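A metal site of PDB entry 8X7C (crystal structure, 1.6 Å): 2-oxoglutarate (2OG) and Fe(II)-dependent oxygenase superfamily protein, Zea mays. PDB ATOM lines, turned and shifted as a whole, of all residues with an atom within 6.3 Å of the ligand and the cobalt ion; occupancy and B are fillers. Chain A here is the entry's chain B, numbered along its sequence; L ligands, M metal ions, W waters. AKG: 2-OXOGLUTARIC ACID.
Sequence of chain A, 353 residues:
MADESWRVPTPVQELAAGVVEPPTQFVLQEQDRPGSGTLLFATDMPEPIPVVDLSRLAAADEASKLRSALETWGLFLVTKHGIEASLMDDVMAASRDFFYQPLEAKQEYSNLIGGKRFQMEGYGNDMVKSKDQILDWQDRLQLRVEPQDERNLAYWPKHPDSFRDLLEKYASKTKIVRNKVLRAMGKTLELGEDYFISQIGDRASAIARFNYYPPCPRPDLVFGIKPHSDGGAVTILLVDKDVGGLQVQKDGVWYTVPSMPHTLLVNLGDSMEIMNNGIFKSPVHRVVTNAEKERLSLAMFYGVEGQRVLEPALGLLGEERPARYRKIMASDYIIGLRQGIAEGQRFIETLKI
OH of Tyr 213 lies within hydrogen-bond range of O4 of the ligand (2.6 Å).
O4 of the ligand lies within hydrogen-bond range of OG of Ser 297, 2.7 Å away.
NH2 of Arg 295 lies within salt-bridge range of O3 of the ligand, 2.8 Å away.
ND2 of Asn 211 is in hydrogen-bond range of O2 of the ligand (3.1 Å).
NE of Arg 209 is in salt-bridge range of O2 of the ligand.
The side-chain carboxylate (OD2) of Asp 230 is in hydrogen-bond range of the side-chain amide nitrogen (ND2) of Asn 267 (3.1 Å).
OG1 of Thr 235 lies within hydrogen-bond range of OD2 of Asp 230.
The backbone carbonyl oxygen (O) of Arg 295 lies within hydrogen-bond range of the backbone NH (N) of Tyr 213, 2.8 Å away.
O of Ser 297 is in hydrogen-bond range of N of Asn 211, 2.8 Å away.
OD1 of Asn 211 lies within hydrogen-bond range of NE of Arg 209, 2.8 Å away.
The side-chain amide nitrogen (NE2) of Gln 138 sits at hydrogen-bond distance from the side-chain amide oxygen (OD1) of Asn 211, 2.8 Å away.
The backbone carbonyl oxygen of Ala 299 lies within hydrogen-bond range of the backbone NH of Arg 209 (2.8 Å).
The backbone NH (N) of Val 287 is in hydrogen-bond range of the backbone carbonyl oxygen (O) of Ile 225 (3.1 Å).
Merely in contact with the ligand: Ile 225 (3.8 Å), Leu 237 (3.4 Å), Leu 246 (3.7 Å), Val 287 (3.5 Å), Ala 299 (3.9 Å) and Phe 301 (3.3 Å).
Hydrophobic or aromatic side chains that line the ligand: Tyr 213, Ile 225, His 228, Leu 237, Leu 246, His 285, Val 287, Ala 299 and Phe 301.
Within 4 Å of the ligand: Arg 209, Asn 211, Tyr 213, Ile 225, His 228, Asp 230, Leu 237, Leu 246, His 285, Val 287, Arg 295, Ser 297, Ala 299 and Phe 301.
The nearest printed residue that does not touch the ligand is Val 239 (4.2 Å).
Three residues have an atom within 4 Å of the cobalt ion: His 228, Asp 230 and His 285.
The nearest printed residue that does not touch the cobalt ion is Phe 301 (4.5 Å).
The cobalt ion is bound by an oxygen (O1) of the ligand (2.1 Å), a ring nitrogen (NE2) of His 228 (2.1 Å), water W2 (2.1 Å), an oxygen (O5) of the ligand (2.1 Å), a ring nitrogen (NE2) of His 285 (2.1 Å) and the side-chain carboxylate of Asp 230 (2.2 Å).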
ATOM      1  N   GLN A 138       7.695   1.056 -27.393  1.00  0.00           N
ATOM      2  CA  GLN A 138       6.392   0.415 -27.223  1.00  0.00           C
ATOM      3  C   GLN A 138       5.314   1.311 -27.794  1.00  0.00           C
ATOM      4  O   GLN A 138       5.509   2.524 -27.953  1.00  0.00           O
ATOM      5  CB  GLN A 138       6.077   0.105 -25.751  1.00  0.00           C
ATOM      6  CG  GLN A 138       5.667   1.346 -24.941  1.00  0.00           C
ATOM      7  CD  GLN A 138       4.708   1.021 -23.794  1.00  0.00           C
ATOM      8  OE1 GLN A 138       4.894   1.482 -22.664  1.00  0.00           O
ATOM      9  NE2 GLN A 138       3.686   0.225 -24.066  1.00  0.00           N
ATOM     10  N   ARG A 209      -4.701  -0.927 -20.054  1.00  0.00           N
ATOM     11  CA  ARG A 209      -3.591  -0.518 -20.923  1.00  0.00           C
ATOM     12  C   ARG A 209      -3.031  -1.757 -21.611  1.00  0.00           C
ATOM     13  O   ARG A 209      -2.430  -2.620 -20.956  1.00  0.00           O
ATOM     14  CB  ARG A 209      -2.518   0.208 -20.126  1.00  0.00           C
ATOM     15  CG  ARG A 209      -1.358   0.699 -21.001  1.00  0.00           C
ATOM     16  CD  ARG A 209      -0.305   1.395 -20.135  1.00  0.00           C
ATOM     17  NE  ARG A 209       0.914   1.686 -20.900  1.00  0.00           N
ATOM     18  CZ  ARG A 209       1.331   2.903 -21.237  1.00  0.00           C
ATOM     19  NH1 ARG A 209       0.633   3.972 -20.857  1.00  0.00           N
ATOM     20  NH2 ARG A 209       2.460   3.051 -21.927  1.00  0.00           N
ATOM     21  N   ASN A 211      -0.259  -3.046 -23.786  1.00  0.00           N
ATOM     22  CA  ASN A 211       1.086  -2.688 -24.223  1.00  0.00           C
ATOM     23  C   ASN A 211       1.563  -3.603 -25.329  1.00  0.00           C
ATOM     24  O   ASN A 211       1.409  -4.830 -25.232  1.00  0.00           O
ATOM     25  CB  ASN A 211       2.073  -2.804 -23.060  1.00  0.00           C
ATOM     26  CG  ASN A 211       1.785  -1.803 -21.965  1.00  0.00           C
ATOM     27  OD1 ASN A 211       1.821  -0.594 -22.186  1.00  0.00           O
ATOM     28  ND2 ASN A 211       1.506  -2.302 -20.756  1.00  0.00           N
ATOM     29  N   TYR A 213       5.167  -4.302 -27.297  1.00  0.00           N
ATOM     30  CA  TYR A 213       6.597  -4.011 -27.392  1.00  0.00           C
ATOM     31  C   TYR A 213       7.155  -4.696 -28.624  1.00  0.00           C
ATOM     32  O   TYR A 213       7.280  -5.923 -28.615  1.00  0.00           O
ATOM     33  CB  TYR A 213       7.355  -4.490 -26.147  1.00  0.00           C
ATOM     34  CG  TYR A 213       6.777  -4.000 -24.858  1.00  0.00           C
ATOM     35  CD1 TYR A 213       7.234  -2.841 -24.263  1.00  0.00           C
ATOM     36  CD2 TYR A 213       5.746  -4.717 -24.231  1.00  0.00           C
ATOM     37  CE1 TYR A 213       6.680  -2.380 -23.044  1.00  0.00           C
ATOM     38  CE2 TYR A 213       5.186  -4.252 -23.029  1.00  0.00           C
ATOM     39  CZ  TYR A 213       5.658  -3.102 -22.448  1.00  0.00           C
ATOM     40  OH  TYR A 213       5.113  -2.647 -21.259  1.00  0.00           O
ATOM     41  N   ILE A 225       9.300  -0.053 -21.516  1.00  0.00           N
ATOM     42  CA  ILE A 225       8.642   1.008 -20.758  1.00  0.00           C
ATOM     43  C   ILE A 225       9.623   1.455 -19.691  1.00  0.00           C
ATOM     44  O   ILE A 225      10.290   0.621 -19.053  1.00  0.00           O
ATOM     45  CB  ILE A 225       7.268   0.578 -20.182  1.00  0.00           C
ATOM     46  CG1 ILE A 225       6.428   1.783 -19.771  1.00  0.00           C
ATOM     47  CG2 ILE A 225       7.368  -0.385 -19.013  1.00  0.00           C
ATOM     48  CD1 ILE A 225       4.964   1.435 -19.427  1.00  0.00           C
ATOM     49  N   HIS A 228       9.174   3.377 -13.733  1.00  0.00           N
ATOM     50  CA  HIS A 228       8.069   4.166 -13.222  1.00  0.00           C
ATOM     51  C   HIS A 228       7.431   3.393 -12.097  1.00  0.00           C
ATOM     52  O   HIS A 228       7.643   2.196 -11.967  1.00  0.00           O
ATOM     53  CB  HIS A 228       7.026   4.436 -14.323  1.00  0.00           C
ATOM     54  CG  HIS A 228       6.293   3.190 -14.758  1.00  0.00           C
ATOM     55  ND1 HIS A 228       6.827   2.282 -15.644  1.00  0.00           N
ATOM     56  CD2 HIS A 228       5.076   2.711 -14.412  1.00  0.00           C
ATOM     57  CE1 HIS A 228       5.972   1.290 -15.820  1.00  0.00           C
ATOM     58  NE2 HIS A 228       4.896   1.535 -15.085  1.00  0.00           N
ATOM     59  N   SER A 229       6.629   4.084 -11.296  1.00  0.00           N
ATOM     60  CA  SER A 229       5.646   3.404 -10.459  1.00  0.00           C
ATOM     61  C   SER A 229       4.268   3.788 -10.970  1.00  0.00           C
ATOM     62  O   SER A 229       4.084   4.853 -11.578  1.00  0.00           O
ATOM     63  CB  SER A 229       5.802   3.759  -8.979  1.00  0.00           C
ATOM     64  OG  SER A 229       5.674   5.162  -8.766  1.00  0.00           O
ATOM     65  N   ASP A 230       3.303   2.893 -10.771  1.00  0.00           N
ATOM     66  CA  ASP A 230       1.933   3.187 -11.192  1.00  0.00           C
ATOM     67  C   ASP A 230       1.293   4.134 -10.172  1.00  0.00           C
ATOM     68  O   ASP A 230       1.621   4.105  -8.991  1.00  0.00           O
ATOM     69  CB  ASP A 230       1.102   1.907 -11.305  1.00  0.00           C
ATOM     70  CG  ASP A 230       1.657   0.909 -12.313  1.00  0.00           C
ATOM     71  OD1 ASP A 230       2.418   1.273 -13.236  1.00  0.00           O
ATOM     72  OD2 ASP A 230       1.287  -0.278 -12.167  1.00  0.00           O
ATOM     73  N   THR A 235      -2.531  -2.560  -9.388  1.00  0.00           N
ATOM     74  CA  THR A 235      -2.491  -2.950 -10.783  1.00  0.00           C
ATOM     75  C   THR A 235      -2.518  -4.469 -10.886  1.00  0.00           C
ATOM     76  O   THR A 235      -1.803  -5.146 -10.154  1.00  0.00           O
ATOM     77  CB  THR A 235      -1.224  -2.439 -11.465  1.00  0.00           C
ATOM     78  OG1 THR A 235      -1.228  -1.007 -11.383  1.00  0.00           O
ATOM     79  CG2 THR A 235      -1.153  -2.882 -12.951  1.00  0.00           C
ATOM     80  N   LEU A 237      -1.754  -7.312 -13.697  1.00  0.00           N
ATOM     81  CA  LEU A 237      -0.996  -7.374 -14.954  1.00  0.00           C
ATOM     82  C   LEU A 237      -1.007  -8.783 -15.534  1.00  0.00           C
ATOM     83  O   LEU A 237      -0.711  -9.742 -14.829  1.00  0.00           O
ATOM     84  CB  LEU A 237       0.462  -6.934 -14.718  1.00  0.00           C
ATOM     85  CG  LEU A 237       1.351  -6.982 -15.962  1.00  0.00           C
ATOM     86  CD1 LEU A 237       1.031  -5.824 -16.921  1.00  0.00           C
ATOM     87  CD2 LEU A 237       2.825  -6.913 -15.521  1.00  0.00           C
ATOM     88  N   LEU A 238      -1.314  -8.875 -16.830  1.00  0.00           N
ATOM     89  CA  LEU A 238      -1.264 -10.107 -17.598  1.00  0.00           C
ATOM     90  C   LEU A 238      -0.218  -9.960 -18.698  1.00  0.00           C
ATOM     91  O   LEU A 238      -0.251  -9.000 -19.471  1.00  0.00           O
ATOM     92  CB  LEU A 238      -2.646 -10.408 -18.200  1.00  0.00           C
ATOM     93  CG  LEU A 238      -2.768 -11.513 -19.241  1.00  0.00           C
ATOM     94  CD1 LEU A 238      -2.392 -12.849 -18.607  1.00  0.00           C
ATOM     95  CD2 LEU A 238      -4.208 -11.548 -19.762  1.00  0.00           C
ATOM     96  N   VAL A 239       0.716 -10.907 -18.770  1.00  0.00           N
ATOM     97  CA  VAL A 239       1.750 -10.910 -19.812  1.00  0.00           C
ATOM     98  C   VAL A 239       1.506 -12.099 -20.715  1.00  0.00           C
ATOM     99  O   VAL A 239       1.527 -13.242 -20.248  1.00  0.00           O
ATOM    100  CB  VAL A 239       3.159 -10.976 -19.208  1.00  0.00           C
ATOM    101  CG1 VAL A 239       4.210 -11.014 -20.333  1.00  0.00           C
ATOM    102  CG2 VAL A 239       3.403  -9.815 -18.229  1.00  0.00           C
ATOM    103  N   GLY A 245      10.753  -9.684 -19.694  1.00  0.00           N
ATOM    104  CA  GLY A 245      10.975  -8.267 -19.935  1.00  0.00           C
ATOM    105  C   GLY A 245      10.744  -7.415 -18.700  1.00  0.00           C
ATOM    106  O   GLY A 245      11.456  -6.418 -18.502  1.00  0.00           O
ATOM    107  N   LEU A 246       9.779  -7.790 -17.863  1.00  0.00           N
ATOM    108  CA  LEU A 246       9.446  -6.984 -16.695  1.00  0.00           C
ATOM    109  C   LEU A 246      10.510  -7.129 -15.610  1.00  0.00           C
ATOM    110  O   LEU A 246      10.931  -8.248 -15.287  1.00  0.00           O
ATOM    111  CB  LEU A 246       8.085  -7.409 -16.129  1.00  0.00           C
ATOM    112  CG  LEU A 246       7.602  -6.620 -14.919  1.00  0.00           C
ATOM    113  CD1 LEU A 246       7.305  -5.162 -15.284  1.00  0.00           C
ATOM    114  CD2 LEU A 246       6.362  -7.306 -14.367  1.00  0.00           C
ATOM    115  N   ASN A 267       0.659  -5.503  -8.444  1.00  0.00           N
ATOM    116  CA  ASN A 267       1.565  -4.561  -7.815  1.00  0.00           C
ATOM    117  C   ASN A 267       0.804  -3.365  -7.253  1.00  0.00           C
ATOM    118  O   ASN A 267      -0.286  -3.019  -7.706  1.00  0.00           O
ATOM    119  CB  ASN A 267       2.689  -4.098  -8.770  1.00  0.00           C
ATOM    120  CG  ASN A 267       2.186  -3.290  -9.937  1.00  0.00           C
ATOM    121  OD1 ASN A 267       1.898  -3.828 -10.997  1.00  0.00           O
ATOM    122  ND2 ASN A 267       2.103  -1.977  -9.754  1.00  0.00           N
ATOM    123  N   HIS A 285       9.137  -0.132 -11.557  1.00  0.00           N
ATOM    124  CA  HIS A 285       9.329  -1.257 -12.457  1.00  0.00           C
ATOM    125  C   HIS A 285       9.566  -0.737 -13.873  1.00  0.00           C
ATOM    126  O   HIS A 285       9.345   0.439 -14.173  1.00  0.00           O
ATOM    127  CB  HIS A 285       8.109  -2.205 -12.374  1.00  0.00           C
ATOM    128  CG  HIS A 285       6.781  -1.523 -12.547  1.00  0.00           C
ATOM    129  ND1 HIS A 285       6.179  -0.778 -11.554  1.00  0.00           N
ATOM    130  CD2 HIS A 285       5.934  -1.505 -13.607  1.00  0.00           C
ATOM    131  CE1 HIS A 285       5.028  -0.317 -11.997  1.00  0.00           C
ATOM    132  NE2 HIS A 285       4.842  -0.743 -13.231  1.00  0.00           N
ATOM    133  N   ARG A 286      10.062  -1.610 -14.743  1.00  0.00           N
ATOM    134  CA  ARG A 286      10.380  -1.266 -16.127  1.00  0.00           C
ATOM    135  C   ARG A 286      10.298  -2.532 -16.968  1.00  0.00           C
ATOM    136  O   ARG A 286      10.245  -3.643 -16.437  1.00  0.00           O
ATOM    137  CB  ARG A 286      11.785  -0.637 -16.255  1.00  0.00           C
ATOM    138  CG  ARG A 286      12.906  -1.659 -16.042  1.00  0.00           C
ATOM    139  CD  ARG A 286      14.282  -1.002 -15.908  1.00  0.00           C
ATOM    140  NE  ARG A 286      15.341  -2.010 -15.939  1.00  0.00           N
ATOM    141  CZ  ARG A 286      16.644  -1.744 -15.787  1.00  0.00           C
ATOM    142  NH1 ARG A 286      17.062  -0.504 -15.586  1.00  0.00           N
ATOM    143  NH2 ARG A 286      17.531  -2.740 -15.834  1.00  0.00           N
ATOM    144  N   VAL A 287      10.288  -2.351 -18.284  1.00  0.00           N
ATOM    145  CA  VAL A 287      10.343  -3.478 -19.218  1.00  0.00           C
ATOM    146  C   VAL A 287      11.514  -3.271 -20.154  1.00  0.00           C
ATOM    147  O   VAL A 287      11.669  -2.190 -20.742  1.00  0.00           O
ATOM    148  CB  VAL A 287       9.028  -3.633 -20.024  1.00  0.00           C
ATOM    149  CG1 VAL A 287       9.213  -4.621 -21.161  1.00  0.00           C
ATOM    150  CG2 VAL A 287       7.903  -4.095 -19.131  1.00  0.00           C
ATOM    151  N   ARG A 295       6.381  -8.497 -27.510  1.00  0.00           N
ATOM    152  CA  ARG A 295       5.856  -8.824 -26.206  1.00  0.00           C
ATOM    153  C   ARG A 295       4.576  -8.031 -26.007  1.00  0.00           C
ATOM    154  O   ARG A 295       4.519  -6.848 -26.364  1.00  0.00           O
ATOM    155  CB  ARG A 295       6.873  -8.499 -25.104  1.00  0.00           C
ATOM    156  CG  ARG A 295       6.392  -8.735 -23.681  1.00  0.00           C
ATOM    157  CD  ARG A 295       7.519  -8.332 -22.707  1.00  0.00           C
ATOM    158  NE  ARG A 295       7.195  -8.604 -21.318  1.00  0.00           N
ATOM    159  CZ  ARG A 295       6.465  -7.797 -20.560  1.00  0.00           C
ATOM    160  NH1 ARG A 295       5.991  -6.665 -21.087  1.00  0.00           N
ATOM    161  NH2 ARG A 295       6.208  -8.090 -19.280  1.00  0.00           N
ATOM    162  N   LEU A 296       3.549  -8.684 -25.474  1.00  0.00           N
ATOM    163  CA  LEU A 296       2.236  -8.074 -25.242  1.00  0.00           C
ATOM    164  C   LEU A 296       1.843  -8.221 -23.780  1.00  0.00           C
ATOM    165  O   LEU A 296       1.961  -9.303 -23.197  1.00  0.00           O
ATOM    166  CB  LEU A 296       1.147  -8.718 -26.102  1.00  0.00           C
ATOM    167  CG  LEU A 296       1.145  -8.316 -27.578  1.00  0.00           C
ATOM    168  CD1 LEU A 296       2.203  -9.052 -28.387  1.00  0.00           C
ATOM    169  CD2 LEU A 296      -0.206  -8.536 -28.192  1.00  0.00           C
ATOM    170  N   SER A 297       1.349  -7.131 -23.187  1.00  0.00           N
ATOM    171  CA  SER A 297       0.821  -7.220 -21.840  1.00  0.00           C
ATOM    172  C   SER A 297      -0.455  -6.409 -21.757  1.00  0.00           C
ATOM    173  O   SER A 297      -0.734  -5.549 -22.604  1.00  0.00           O
ATOM    174  CB  SER A 297       1.833  -6.722 -20.778  1.00  0.00           C
ATOM    175  OG  SER A 297       2.046  -5.314 -20.886  1.00  0.00           O
ATOM    176  N   LEU A 298      -1.236  -6.697 -20.716  1.00  0.00           N
ATOM    177  CA  LEU A 298      -2.452  -5.947 -20.411  1.00  0.00           C
ATOM    178  C   LEU A 298      -2.411  -5.591 -18.934  1.00  0.00           C
ATOM    179  O   LEU A 298      -2.426  -6.491 -18.080  1.00  0.00           O
ATOM    180  CB  LEU A 298      -3.699  -6.765 -20.734  1.00  0.00           C
ATOM    181  CG  LEU A 298      -5.037  -6.215 -20.212  1.00  0.00           C
ATOM    182  CD1 LEU A 298      -5.253  -4.759 -20.670  1.00  0.00           C
ATOM    183  CD2 LEU A 298      -6.164  -7.095 -20.711  1.00  0.00           C
ATOM    184  N   ALA A 299      -2.349  -4.305 -18.640  1.00  0.00           N
ATOM    185  CA  ALA A 299      -2.366  -3.794 -17.270  1.00  0.00           C
ATOM    186  C   ALA A 299      -3.750  -3.264 -16.968  1.00  0.00           C
ATOM    187  O   ALA A 299      -4.295  -2.462 -17.726  1.00  0.00           O
ATOM    188  CB  ALA A 299      -1.329  -2.684 -17.088  1.00  0.00           C
ATOM    189  N   PHE A 301      -5.335  -0.971 -14.370  1.00  0.00           N
ATOM    190  CA  PHE A 301      -5.009  -0.002 -13.326  1.00  0.00           C
ATOM    191  C   PHE A 301      -6.263   0.307 -12.532  1.00  0.00           C
ATOM    192  O   PHE A 301      -7.225   0.822 -13.086  1.00  0.00           O
ATOM    193  CB  PHE A 301      -4.481   1.309 -13.932  1.00  0.00           C
ATOM    194  CG  PHE A 301      -3.251   1.172 -14.773  1.00  0.00           C
ATOM    195  CD1 PHE A 301      -3.221   1.691 -16.065  1.00  0.00           C
ATOM    196  CD2 PHE A 301      -2.105   0.566 -14.261  1.00  0.00           C
ATOM    197  CE1 PHE A 301      -2.073   1.594 -16.848  1.00  0.00           C
ATOM    198  CE2 PHE A 301      -0.952   0.460 -15.061  1.00  0.00           C
ATOM    199  CZ  PHE A 301      -0.946   0.987 -16.342  1.00  0.00           C
HETATM  200  C1  AKG L   1       2.430  -0.403 -17.238  1.00  0.00           C
HETATM  201  O1  AKG L   1       2.330   0.483 -16.362  1.00  0.00           O
HETATM  202  O2  AKG L   1       1.682  -0.470 -18.265  1.00  0.00           O
HETATM  203  C2  AKG L   1       3.487  -1.464 -17.048  1.00  0.00           C
HETATM  204  O5  AKG L   1       4.241  -1.356 -16.115  1.00  0.00           O
HETATM  205  C3  AKG L   1       3.560  -2.616 -18.069  1.00  0.00           C
HETATM  206  C4  AKG L   1       4.468  -3.697 -17.498  1.00  0.00           C
HETATM  207  C5  AKG L   1       4.588  -4.824 -18.506  1.00  0.00           C
HETATM  208  O3  AKG L   1       4.903  -5.937 -18.043  1.00  0.00           O
HETATM  209  O4  AKG L   1       4.389  -4.673 -19.748  1.00  0.00           O
HETATM  210 CO    CO M   1       3.478   0.034 -14.693  1.00  0.00          CO
HETATM  211  O   HOH W   1       1.658   3.478 -14.853  1.00  0.00           O
HETATM  212  O   HOH W   2       2.159  -1.551 -14.267  1.00  0.00           O
HETATM  213  O   HOH W   3       1.769   2.883 -17.329  1.00  0.00           O
